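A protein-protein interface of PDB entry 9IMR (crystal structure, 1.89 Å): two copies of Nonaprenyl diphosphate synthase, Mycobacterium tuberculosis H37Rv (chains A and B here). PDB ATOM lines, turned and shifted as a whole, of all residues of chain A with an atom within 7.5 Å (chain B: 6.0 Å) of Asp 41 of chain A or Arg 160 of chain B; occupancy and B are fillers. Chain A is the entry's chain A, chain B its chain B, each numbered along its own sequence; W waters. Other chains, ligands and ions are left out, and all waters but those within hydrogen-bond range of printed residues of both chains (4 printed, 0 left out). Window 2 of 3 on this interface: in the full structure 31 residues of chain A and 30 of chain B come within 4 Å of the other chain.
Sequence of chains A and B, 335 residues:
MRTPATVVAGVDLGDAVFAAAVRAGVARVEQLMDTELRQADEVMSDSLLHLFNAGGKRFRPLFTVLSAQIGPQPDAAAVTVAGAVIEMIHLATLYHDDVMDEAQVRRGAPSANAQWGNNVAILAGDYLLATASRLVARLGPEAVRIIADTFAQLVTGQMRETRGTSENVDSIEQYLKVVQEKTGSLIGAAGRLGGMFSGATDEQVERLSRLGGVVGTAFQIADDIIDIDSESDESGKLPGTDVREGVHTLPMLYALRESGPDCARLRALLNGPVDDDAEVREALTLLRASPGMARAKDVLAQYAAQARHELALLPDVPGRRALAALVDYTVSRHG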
ATOM      1  N   LEU A  37      11.940   6.595  21.658  1.00  0.00           N
ATOM      2  CA  LEU A  37      12.667   7.818  21.236  1.00  0.00           C
ATOM      3  C   LEU A  37      14.180   7.559  21.236  1.00  0.00           C
ATOM      4  O   LEU A  37      14.892   8.126  20.344  1.00  0.00           O
ATOM      5  CB  LEU A  37      12.313   8.969  22.172  1.00  0.00           C
ATOM      6  CG  LEU A  37      10.858   9.417  22.107  1.00  0.00           C
ATOM      7  CD1 LEU A  37      10.653  10.490  23.119  1.00  0.00           C
ATOM      8  CD2 LEU A  37      10.501   9.934  20.726  1.00  0.00           C
ATOM      9  N   ARG A  38      14.660   6.712  22.150  1.00  0.00           N
ATOM     10  CA  ARG A  38      16.122   6.473  22.343  1.00  0.00           C
ATOM     11  C   ARG A  38      16.630   5.419  21.353  1.00  0.00           C
ATOM     12  O   ARG A  38      17.833   5.246  21.289  1.00  0.00           O
ATOM     13  CB  ARG A  38      16.402   6.087  23.798  1.00  0.00           C
ATOM     14  CG  ARG A  38      16.331   7.272  24.744  1.00  0.00           C
ATOM     15  CD  ARG A  38      16.454   6.934  26.215  1.00  0.00           C
ATOM     16  NE  ARG A  38      16.213   8.096  27.075  1.00  0.00           N
ATOM     17  CZ  ARG A  38      17.068   9.094  27.279  1.00  0.00           C
ATOM     18  NH1 ARG A  38      18.266   9.104  26.710  1.00  0.00           N
ATOM     19  NH2 ARG A  38      16.722  10.095  28.061  1.00  0.00           N
ATOM     20  N   GLN A  39      15.778   4.760  20.586  1.00  0.00           N
ATOM     21  CA  GLN A  39      16.197   3.770  19.560  1.00  0.00           C
ATOM     22  C   GLN A  39      16.595   4.476  18.259  1.00  0.00           C
ATOM     23  O   GLN A  39      17.179   3.825  17.385  1.00  0.00           O
ATOM     24  CB  GLN A  39      15.082   2.765  19.298  1.00  0.00           C
ATOM     25  CG  GLN A  39      14.784   1.895  20.510  1.00  0.00           C
ATOM     26  CD  GLN A  39      15.417   0.530  20.432  1.00  0.00           C
ATOM     27  OE1 GLN A  39      15.748   0.046  19.352  1.00  0.00           O
ATOM     28  NE2 GLN A  39      15.546  -0.117  21.583  1.00  0.00           N
ATOM     29  N   ALA A  40      16.301   5.764  18.110  1.00  0.00           N
ATOM     30  CA  ALA A  40      16.593   6.497  16.859  1.00  0.00           C
ATOM     31  C   ALA A  40      18.109   6.643  16.686  1.00  0.00           C
ATOM     32  O   ALA A  40      18.847   6.688  17.673  1.00  0.00           O
ATOM     33  CB  ALA A  40      15.888   7.829  16.875  1.00  0.00           C
ATOM     34  N   ASP A  41      18.561   6.755  15.450  1.00  0.00           N
ATOM     35  CA  ASP A  41      19.962   7.130  15.150  1.00  0.00           C
ATOM     36  C   ASP A  41      20.380   8.314  16.024  1.00  0.00           C
ATOM     37  O   ASP A  41      19.572   9.252  16.185  1.00  0.00           O
ATOM     38  CB  ASP A  41      20.089   7.468  13.674  1.00  0.00           C
ATOM     39  CG  ASP A  41      21.515   7.683  13.194  1.00  0.00           C
ATOM     40  OD1 ASP A  41      22.134   8.697  13.542  1.00  0.00           O
ATOM     41  OD2 ASP A  41      21.956   6.862  12.399  1.00  0.00           O
ATOM     42  N   GLU A  42      21.625   8.313  16.498  1.00  0.00           N
ATOM     43  CA  GLU A  42      22.251   9.427  17.271  1.00  0.00           C
ATOM     44  C   GLU A  42      21.920  10.797  16.654  1.00  0.00           C
ATOM     45  O   GLU A  42      21.812  11.753  17.403  1.00  0.00           O
ATOM     46  CB  GLU A  42      23.764   9.169  17.310  1.00  0.00           C
ATOM     47  CG  GLU A  42      24.626  10.382  17.578  1.00  0.00           C
ATOM     48  CD  GLU A  42      25.089  11.221  16.381  1.00  0.00           C
ATOM     49  OE1 GLU A  42      25.158  12.468  16.552  1.00  0.00           O
ATOM     50  OE2 GLU A  42      25.421  10.652  15.287  1.00  0.00           O
ATOM     51  N   VAL A  43      21.886  10.935  15.323  1.00  0.00           N
ATOM     52  CA  VAL A  43      21.671  12.251  14.653  1.00  0.00           C
ATOM     53  C   VAL A  43      20.310  12.837  15.029  1.00  0.00           C
ATOM     54  O   VAL A  43      20.183  14.077  15.082  1.00  0.00           O
ATOM     55  CB  VAL A  43      21.863  12.130  13.132  1.00  0.00           C
ATOM     56  CG1 VAL A  43      20.652  11.579  12.422  1.00  0.00           C
ATOM     57  CG2 VAL A  43      22.241  13.478  12.585  1.00  0.00           C
ATOM     58  N   MET A  44      19.350  11.976  15.348  1.00  0.00           N
ATOM     59  CA  MET A  44      17.964  12.348  15.745  1.00  0.00           C
ATOM     60  C   MET A  44      17.859  12.611  17.257  1.00  0.00           C
ATOM     61  O   MET A  44      16.903  13.271  17.674  1.00  0.00           O
ATOM     62  CB  MET A  44      17.020  11.201  15.392  1.00  0.00           C
ATOM     63  CG  MET A  44      16.893  10.924  13.928  1.00  0.00           C
ATOM     64  SD  MET A  44      16.451  12.376  12.946  1.00  0.00           S
ATOM     65  CE  MET A  44      14.985  12.920  13.810  1.00  0.00           C
ATOM     66  N   SER A  45      18.786  12.094  18.074  1.00  0.00           N
ATOM     67  CA  SER A  45      18.550  11.842  19.515  1.00  0.00           C
ATOM     68  C   SER A  45      18.229  13.143  20.265  1.00  0.00           C
ATOM     69  O   SER A  45      17.155  13.174  20.948  1.00  0.00           O
ATOM     70  CB  SER A  45      19.708  11.054  20.132  1.00  0.00           C
ATOM     71  OG  SER A  45      19.722  11.291  21.527  1.00  0.00           O
ATOM     72  N   ASP A  46      19.044  14.197  20.103  1.00  0.00           N
ATOM     73  CA  ASP A  46      18.895  15.481  20.832  1.00  0.00           C
ATOM     74  C   ASP A  46      17.503  16.054  20.524  1.00  0.00           C
ATOM     75  O   ASP A  46      16.799  16.543  21.452  1.00  0.00           O
ATOM     76  CB  ASP A  46      19.946  16.514  20.422  1.00  0.00           C
ATOM     77  CG  ASP A  46      21.362  16.263  20.944  1.00  0.00           C
ATOM     78  OD1 ASP A  46      21.544  15.347  21.738  1.00  0.00           O
ATOM     79  OD2 ASP A  46      22.260  16.955  20.481  1.00  0.00           O
ATOM     80  N   LEU A  48      14.778  14.605  19.234  1.00  0.00           N
ATOM     81  CA  LEU A  48      13.635  13.707  19.580  1.00  0.00           C
ATOM     82  C   LEU A  48      13.373  13.738  21.072  1.00  0.00           C
ATOM     83  O   LEU A  48      12.256  13.469  21.446  1.00  0.00           O
ATOM     84  CB  LEU A  48      13.922  12.259  19.179  1.00  0.00           C
ATOM     85  CG  LEU A  48      13.797  11.949  17.698  1.00  0.00           C
ATOM     86  CD1 LEU A  48      14.024  10.459  17.470  1.00  0.00           C
ATOM     87  CD2 LEU A  48      12.451  12.419  17.149  1.00  0.00           C
ATOM     88  N   LEU A 123      11.934  18.175  10.735  1.00  0.00           N
ATOM     89  CA  LEU A 123      12.374  16.777  10.529  1.00  0.00           C
ATOM     90  C   LEU A 123      12.146  15.965  11.805  1.00  0.00           C
ATOM     91  O   LEU A 123      11.706  14.802  11.709  1.00  0.00           O
ATOM     92  CB  LEU A 123      13.853  16.817  10.157  1.00  0.00           C
ATOM     93  CG  LEU A 123      14.130  17.337   8.756  1.00  0.00           C
ATOM     94  CD1 LEU A 123      15.601  17.464   8.540  1.00  0.00           C
ATOM     95  CD2 LEU A 123      13.517  16.473   7.664  1.00  0.00           C
ATOM     96  N   TYR A 127       9.954  12.581  11.797  1.00  0.00           N
ATOM     97  CA  TYR A 127      10.497  11.326  12.363  1.00  0.00           C
ATOM     98  C   TYR A 127       9.483  10.710  13.350  1.00  0.00           C
ATOM     99  O   TYR A 127       9.275   9.475  13.296  1.00  0.00           O
ATOM    100  CB  TYR A 127      11.830  11.565  13.064  1.00  0.00           C
ATOM    101  CG  TYR A 127      12.536  10.262  13.319  1.00  0.00           C
ATOM    102  CD1 TYR A 127      12.210   9.509  14.434  1.00  0.00           C
ATOM    103  CD2 TYR A 127      13.476   9.746  12.433  1.00  0.00           C
ATOM    104  CE1 TYR A 127      12.830   8.298  14.701  1.00  0.00           C
ATOM    105  CE2 TYR A 127      14.062   8.520  12.666  1.00  0.00           C
ATOM    106  CZ  TYR A 127      13.755   7.807  13.809  1.00  0.00           C
ATOM    107  OH  TYR A 127      14.335   6.629  14.101  1.00  0.00           O
ATOM    108  N   VAL B 155      14.113  10.494   6.709  1.00  0.00           N
ATOM    109  CA  VAL B 155      14.200  11.665   7.611  1.00  0.00           C
ATOM    110  C   VAL B 155      15.576  11.711   8.279  1.00  0.00           C
ATOM    111  O   VAL B 155      16.094  12.817   8.472  1.00  0.00           O
ATOM    112  CB  VAL B 155      13.027  11.654   8.606  1.00  0.00           C
ATOM    113  CG1 VAL B 155      13.173  12.732   9.661  1.00  0.00           C
ATOM    114  CG2 VAL B 155      11.728  11.827   7.849  1.00  0.00           C
ATOM    115  N   THR B 156      16.133  10.563   8.655  1.00  0.00           N
ATOM    116  CA  THR B 156      17.485  10.498   9.250  1.00  0.00           C
ATOM    117  C   THR B 156      18.474  11.139   8.262  1.00  0.00           C
ATOM    118  O   THR B 156      19.277  11.952   8.709  1.00  0.00           O
ATOM    119  CB  THR B 156      17.863   9.075   9.687  1.00  0.00           C
ATOM    120  OG1 THR B 156      16.877   8.617  10.618  1.00  0.00           O
ATOM    121  CG2 THR B 156      19.229   9.072  10.328  1.00  0.00           C
ATOM    122  N   GLY B 157      18.344  10.855   6.971  1.00  0.00           N
ATOM    123  CA  GLY B 157      19.227  11.428   5.947  1.00  0.00           C
ATOM    124  C   GLY B 157      19.084  12.946   5.895  1.00  0.00           C
ATOM    125  O   GLY B 157      20.077  13.668   5.844  1.00  0.00           O
ATOM    126  N   GLN B 158      17.862  13.418   5.804  1.00  0.00           N
ATOM    127  CA  GLN B 158      17.565  14.867   5.801  1.00  0.00           C
ATOM    128  C   GLN B 158      18.196  15.521   7.032  1.00  0.00           C
ATOM    129  O   GLN B 158      18.741  16.618   6.876  1.00  0.00           O
ATOM    130  CB  GLN B 158      16.048  15.067   5.727  1.00  0.00           C
ATOM    131  CG  GLN B 158      15.399  14.748   4.383  1.00  0.00           C
ATOM    132  CD  GLN B 158      15.606  15.762   3.276  1.00  0.00           C
ATOM    133  OE1 GLN B 158      14.698  16.542   2.880  1.00  0.00           O
ATOM    134  NE2 GLN B 158      16.829  15.803   2.791  1.00  0.00           N
ATOM    135  N   MET B 159      18.094  14.880   8.210  1.00  0.00           N
ATOM    136  CA  MET B 159      18.570  15.432   9.496  1.00  0.00           C
ATOM    137  C   MET B 159      20.093  15.425   9.472  1.00  0.00           C
ATOM    138  O   MET B 159      20.689  16.425   9.836  1.00  0.00           O
ATOM    139  CB  MET B 159      18.062  14.643  10.713  1.00  0.00           C
ATOM    140  CG  MET B 159      18.468  15.272  12.033  1.00  0.00           C
ATOM    141  SD  MET B 159      17.672  16.877  12.336  1.00  0.00           S
ATOM    142  CE  MET B 159      16.128  16.318  13.043  1.00  0.00           C
ATOM    143  N   ARG B 160      20.682  14.325   9.024  1.00  0.00           N
ATOM    144  CA  ARG B 160      22.142  14.174   8.904  1.00  0.00           C
ATOM    145  C   ARG B 160      22.685  15.289   8.024  1.00  0.00           C
ATOM    146  O   ARG B 160      23.660  15.964   8.428  1.00  0.00           O
ATOM    147  CB  ARG B 160      22.493  12.775   8.400  1.00  0.00           C
ATOM    148  CG  ARG B 160      23.972  12.484   8.569  1.00  0.00           C
ATOM    149  CD  ARG B 160      24.392  11.179   7.949  1.00  0.00           C
ATOM    150  NE  ARG B 160      23.634  10.072   8.474  1.00  0.00           N
ATOM    151  CZ  ARG B 160      23.805   9.528   9.674  1.00  0.00           C
ATOM    152  NH1 ARG B 160      24.681  10.037  10.518  1.00  0.00           N
ATOM    153  NH2 ARG B 160      23.039   8.511  10.045  1.00  0.00           N
ATOM    154  N   GLU B 161      22.013  15.562   6.914  1.00  0.00           N
ATOM    155  CA  GLU B 161      22.419  16.661   6.028  1.00  0.00           C
ATOM    156  C   GLU B 161      22.356  18.030   6.748  1.00  0.00           C
ATOM    157  O   GLU B 161      23.268  18.858   6.558  1.00  0.00           O
ATOM    158  CB  GLU B 161      21.495  16.652   4.824  1.00  0.00           C
ATOM    159  CG  GLU B 161      21.834  17.728   3.840  1.00  0.00           C
ATOM    160  CD  GLU B 161      20.929  17.653   2.640  1.00  0.00           C
ATOM    161  OE1 GLU B 161      19.958  18.416   2.628  1.00  0.00           O
ATOM    162  OE2 GLU B 161      21.175  16.777   1.751  1.00  0.00           O
ATOM    163  N   THR B 162      21.306  18.323   7.504  1.00  0.00           N
ATOM    164  CA  THR B 162      21.135  19.669   8.129  1.00  0.00           C
ATOM    165  C   THR B 162      22.168  19.868   9.235  1.00  0.00           C
ATOM    166  O   THR B 162      22.696  20.978   9.350  1.00  0.00           O
ATOM    167  CB  THR B 162      19.788  19.893   8.829  1.00  0.00           C
ATOM    168  OG1 THR B 162      19.938  19.205  10.066  1.00  0.00           O
ATOM    169  CG2 THR B 162      18.621  19.377   8.055  1.00  0.00           C
ATOM    170  N   ARG B 163      22.430  18.833  10.035  1.00  0.00           N
ATOM    171  CA  ARG B 163      23.416  18.921  11.145  1.00  0.00           C
ATOM    172  C   ARG B 163      24.783  19.151  10.491  1.00  0.00           C
ATOM    173  O   ARG B 163      25.526  20.071  10.893  1.00  0.00           O
ATOM    174  CB  ARG B 163      23.408  17.655  12.007  1.00  0.00           C
ATOM    175  CG  ARG B 163      22.135  17.408  12.807  1.00  0.00           C
ATOM    176  CD  ARG B 163      21.477  18.617  13.443  1.00  0.00           C
ATOM    177  NE  ARG B 163      20.534  18.197  14.486  1.00  0.00           N
ATOM    178  CZ  ARG B 163      20.569  18.581  15.768  1.00  0.00           C
ATOM    179  NH1 ARG B 163      19.665  18.136  16.633  1.00  0.00           N
ATOM    180  NH2 ARG B 163      21.505  19.420  16.180  1.00  0.00           N
ATOM    181  N   GLY B 164      25.096  18.366   9.473  1.00  0.00           N
ATOM    182  CA  GLY B 164      26.141  18.755   8.513  1.00  0.00           C
ATOM    183  C   GLY B 164      25.850  20.131   7.957  1.00  0.00           C
ATOM    184  O   GLY B 164      26.807  20.910   7.916  1.00  0.00           O
ATOM    185  N   GLN B 174      30.178  11.120   5.196  1.00  0.00           N
ATOM    186  CA  GLN B 174      28.889  11.586   5.766  1.00  0.00           C
ATOM    187  C   GLN B 174      27.918  11.837   4.606  1.00  0.00           C
ATOM    188  O   GLN B 174      26.734  11.415   4.688  1.00  0.00           O
ATOM    189  CB  GLN B 174      29.088  12.816   6.645  1.00  0.00           C
ATOM    190  CG  GLN B 174      27.786  13.388   7.132  1.00  0.00           C
ATOM    191  CD  GLN B 174      27.968  14.513   8.122  1.00  0.00           C
ATOM    192  OE1 GLN B 174      28.353  15.630   7.767  1.00  0.00           O
ATOM    193  NE2 GLN B 174      27.652  14.222   9.366  1.00  0.00           N
ATOM    194  N   LYS B 177      26.495   8.700   3.287  1.00  0.00           N
ATOM    195  CA  LYS B 177      25.455   8.128   4.188  1.00  0.00           C
ATOM    196  C   LYS B 177      24.152   8.925   4.045  1.00  0.00           C
ATOM    197  O   LYS B 177      23.066   8.331   3.917  1.00  0.00           O
ATOM    198  CB  LYS B 177      25.985   8.131   5.612  1.00  0.00           C
ATOM    199  CG  LYS B 177      25.131   7.345   6.584  1.00  0.00           C
ATOM    200  CD  LYS B 177      25.908   6.759   7.737  1.00  0.00           C
ATOM    201  CE  LYS B 177      26.911   7.726   8.332  1.00  0.00           C
ATOM    202  NZ  LYS B 177      28.029   7.010   8.990  1.00  0.00           N
ATOM    203  N   VAL B 178      24.270  10.247   3.987  1.00  0.00           N
ATOM    204  CA  VAL B 178      23.113  11.159   3.737  1.00  0.00           C
ATOM    205  C   VAL B 178      22.348  10.682   2.512  1.00  0.00           C
ATOM    206  O   VAL B 178      21.117  10.557   2.570  1.00  0.00           O
ATOM    207  CB  VAL B 178      23.553  12.623   3.560  1.00  0.00           C
ATOM    208  CG1 VAL B 178      22.412  13.492   2.981  1.00  0.00           C
ATOM    209  CG2 VAL B 178      24.109  13.216   4.849  1.00  0.00           C
ATOM    210  N   GLU B 181      20.536   7.349   2.702  1.00  0.00           N
ATOM    211  CA  GLU B 181      19.365   7.517   3.608  1.00  0.00           C
ATOM    212  C   GLU B 181      18.255   8.328   2.942  1.00  0.00           C
ATOM    213  O   GLU B 181      17.121   7.801   2.836  1.00  0.00           O
ATOM    214  CB  GLU B 181      19.793   8.142   4.931  1.00  0.00           C
ATOM    215  CG  GLU B 181      20.581   7.213   5.829  1.00  0.00           C
ATOM    216  CD  GLU B 181      21.257   7.932   6.987  1.00  0.00           C
ATOM    217  OE1 GLU B 181      21.431   9.176   6.894  1.00  0.00           O
ATOM    218  OE2 GLU B 181      21.631   7.254   7.980  1.00  0.00           O
HETATM  219  O   HOH W   1      17.169   6.725  12.906  1.00  0.00           O
HETATM  220  O   HOH W   2      18.796  15.742  16.782  1.00  0.00           O
HETATM  221  O   HOH W   3      22.386  15.972  16.447  1.00  0.00           O
HETATM  222  O   HOH W   4      24.889   8.752  13.022  1.00  0.00           O
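Asp 41 of chain A touches two residues of chain B.
Arg 160 of chain B touches just these residues of chain A: Asp 41 and Val 43.
Printed residues of chain A within 4 Å of Arg 163 of chain B: Val 43.
Of the printed residues of chain A, Thr 156 of chain B touches Asp 41, Val 43 and Tyr 127.
Of the printed residues of chain A, Gln 158 of chain B touches Leu 123 (3.5 Å).
Printed residues of chain B within 4 Å of Val 43 of chain A: Thr 156, Met 159, Arg 160 and Arg 163.
Of the printed residues of chain B, Leu 123 of chain A touches Val 155, Gln 158, Met 159 and Thr 162.
Glu 161 of chain B touches none of the printed residues of chain A.
Gly 164 of chain B touches none of the printed residues of chain A.
The nearest residue of chain A that does not touch Arg 160 of chain B is Glu 42 of chain A (4.9 Å).
The nearest printed residue of chain A that does not touch Gln 158 of chain B is Met 44 of chain A (6.9 Å).
OD2 of Asp 41 of chain A is in salt-bridge range of NH2 of Arg 160 of chain B.
No position is printed for both chains.
Of the 13 pairs that touch across the chains among the printed residues, none has its exchanged pair printed and touching as well.
Of the 14 printed residues of chain B, 7 touch a printed residue of chain A.
Hydrophobic or aromatic side chains of chain B within 4 Å of the printed part of chain A: Val 155 and Met 159.
Of the 13 printed residues of chain A, 5 touch a printed residue of chain B.
Printed residues of chain A that touch a printed residue of chain B: Asp 41, Val 43, Met 44, Leu 123 and Tyr 127.
Hydrophobic or aromatic side chains of chain A within 4 Å of the printed part of chain B: Val 43, Met 44, Leu 123 and Tyr 127.
Among the printed residues, Asp or Glu carboxylates within 4 Å of a Lys or Arg side-chain nitrogen of the other chain: Asp 41 of chain A with Arg 160 of chain B (3.1 Å).
Water W2 lies within hydrogen-bond range of the guanidinium group (NH1) of Arg 163 of chain B, the backbone carbonyl oxygen (O) of Val 43 of chain A and the backbone carbonyl oxygen (O) of Met 44 of chain A.
Water W4 lies within hydrogen-bond range of OD1 of Asp 41 of chain A (2.8 Å), NH1 of Arg 160 of chain B (2.8 Å) and OE2 of Glu 42 of chain A (3.0 Å).
Water W1 lies within hydrogen-bond range of the backbone NH of Asp 41 of chain A, the side-chain hydroxyl of Thr 156 of chain B and the side-chain hydroxyl of Tyr 127 of chain A.
Water W3 bridges the backbone carbonyl oxygen (O) of Val 43 of chain A and the guanidinium group (NH1) of Arg 163 of chain B.
OD1 of Asp 41 of chain A lies within hydrogen-bond range of N of Val 43 of chain A (2.9 Å).
The backbone carbonyl oxygen (O) of Met 159 of chain B lies within hydrogen-bond range of the side-chain hydroxyl (OG1) of Thr 162 of chain B (2.9 Å).
NH2 of Arg 160 of chain B lies within salt-bridge range of OE2 of Glu 181 of chain B, at 2.8 Å.
Among the printed residues, pairs that only touch across the chains: Leu 123 of chain A with Val 155 of chain B, Tyr 127 of chain A with Thr 156 of chain B, Leu 123 of chain A with Gln 158 of chain B, Val 43 of chain A with Thr 156 of chain B, Met 44 of chain A with Met 159 of chain B, Leu 123 of chain A with Met 159 of chain B, Leu 123 of chain A with Thr 162 of chain B, Val 43 of chain A with Met 159 of chain B, Val 43 of chain A with Arg 160 of chain B, Asp 41 of chain A with Thr 156 of chain B, Tyr 127 of chain A with Val 155 of chain B and Val 43 of chain A with Arg 163 of chain B.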
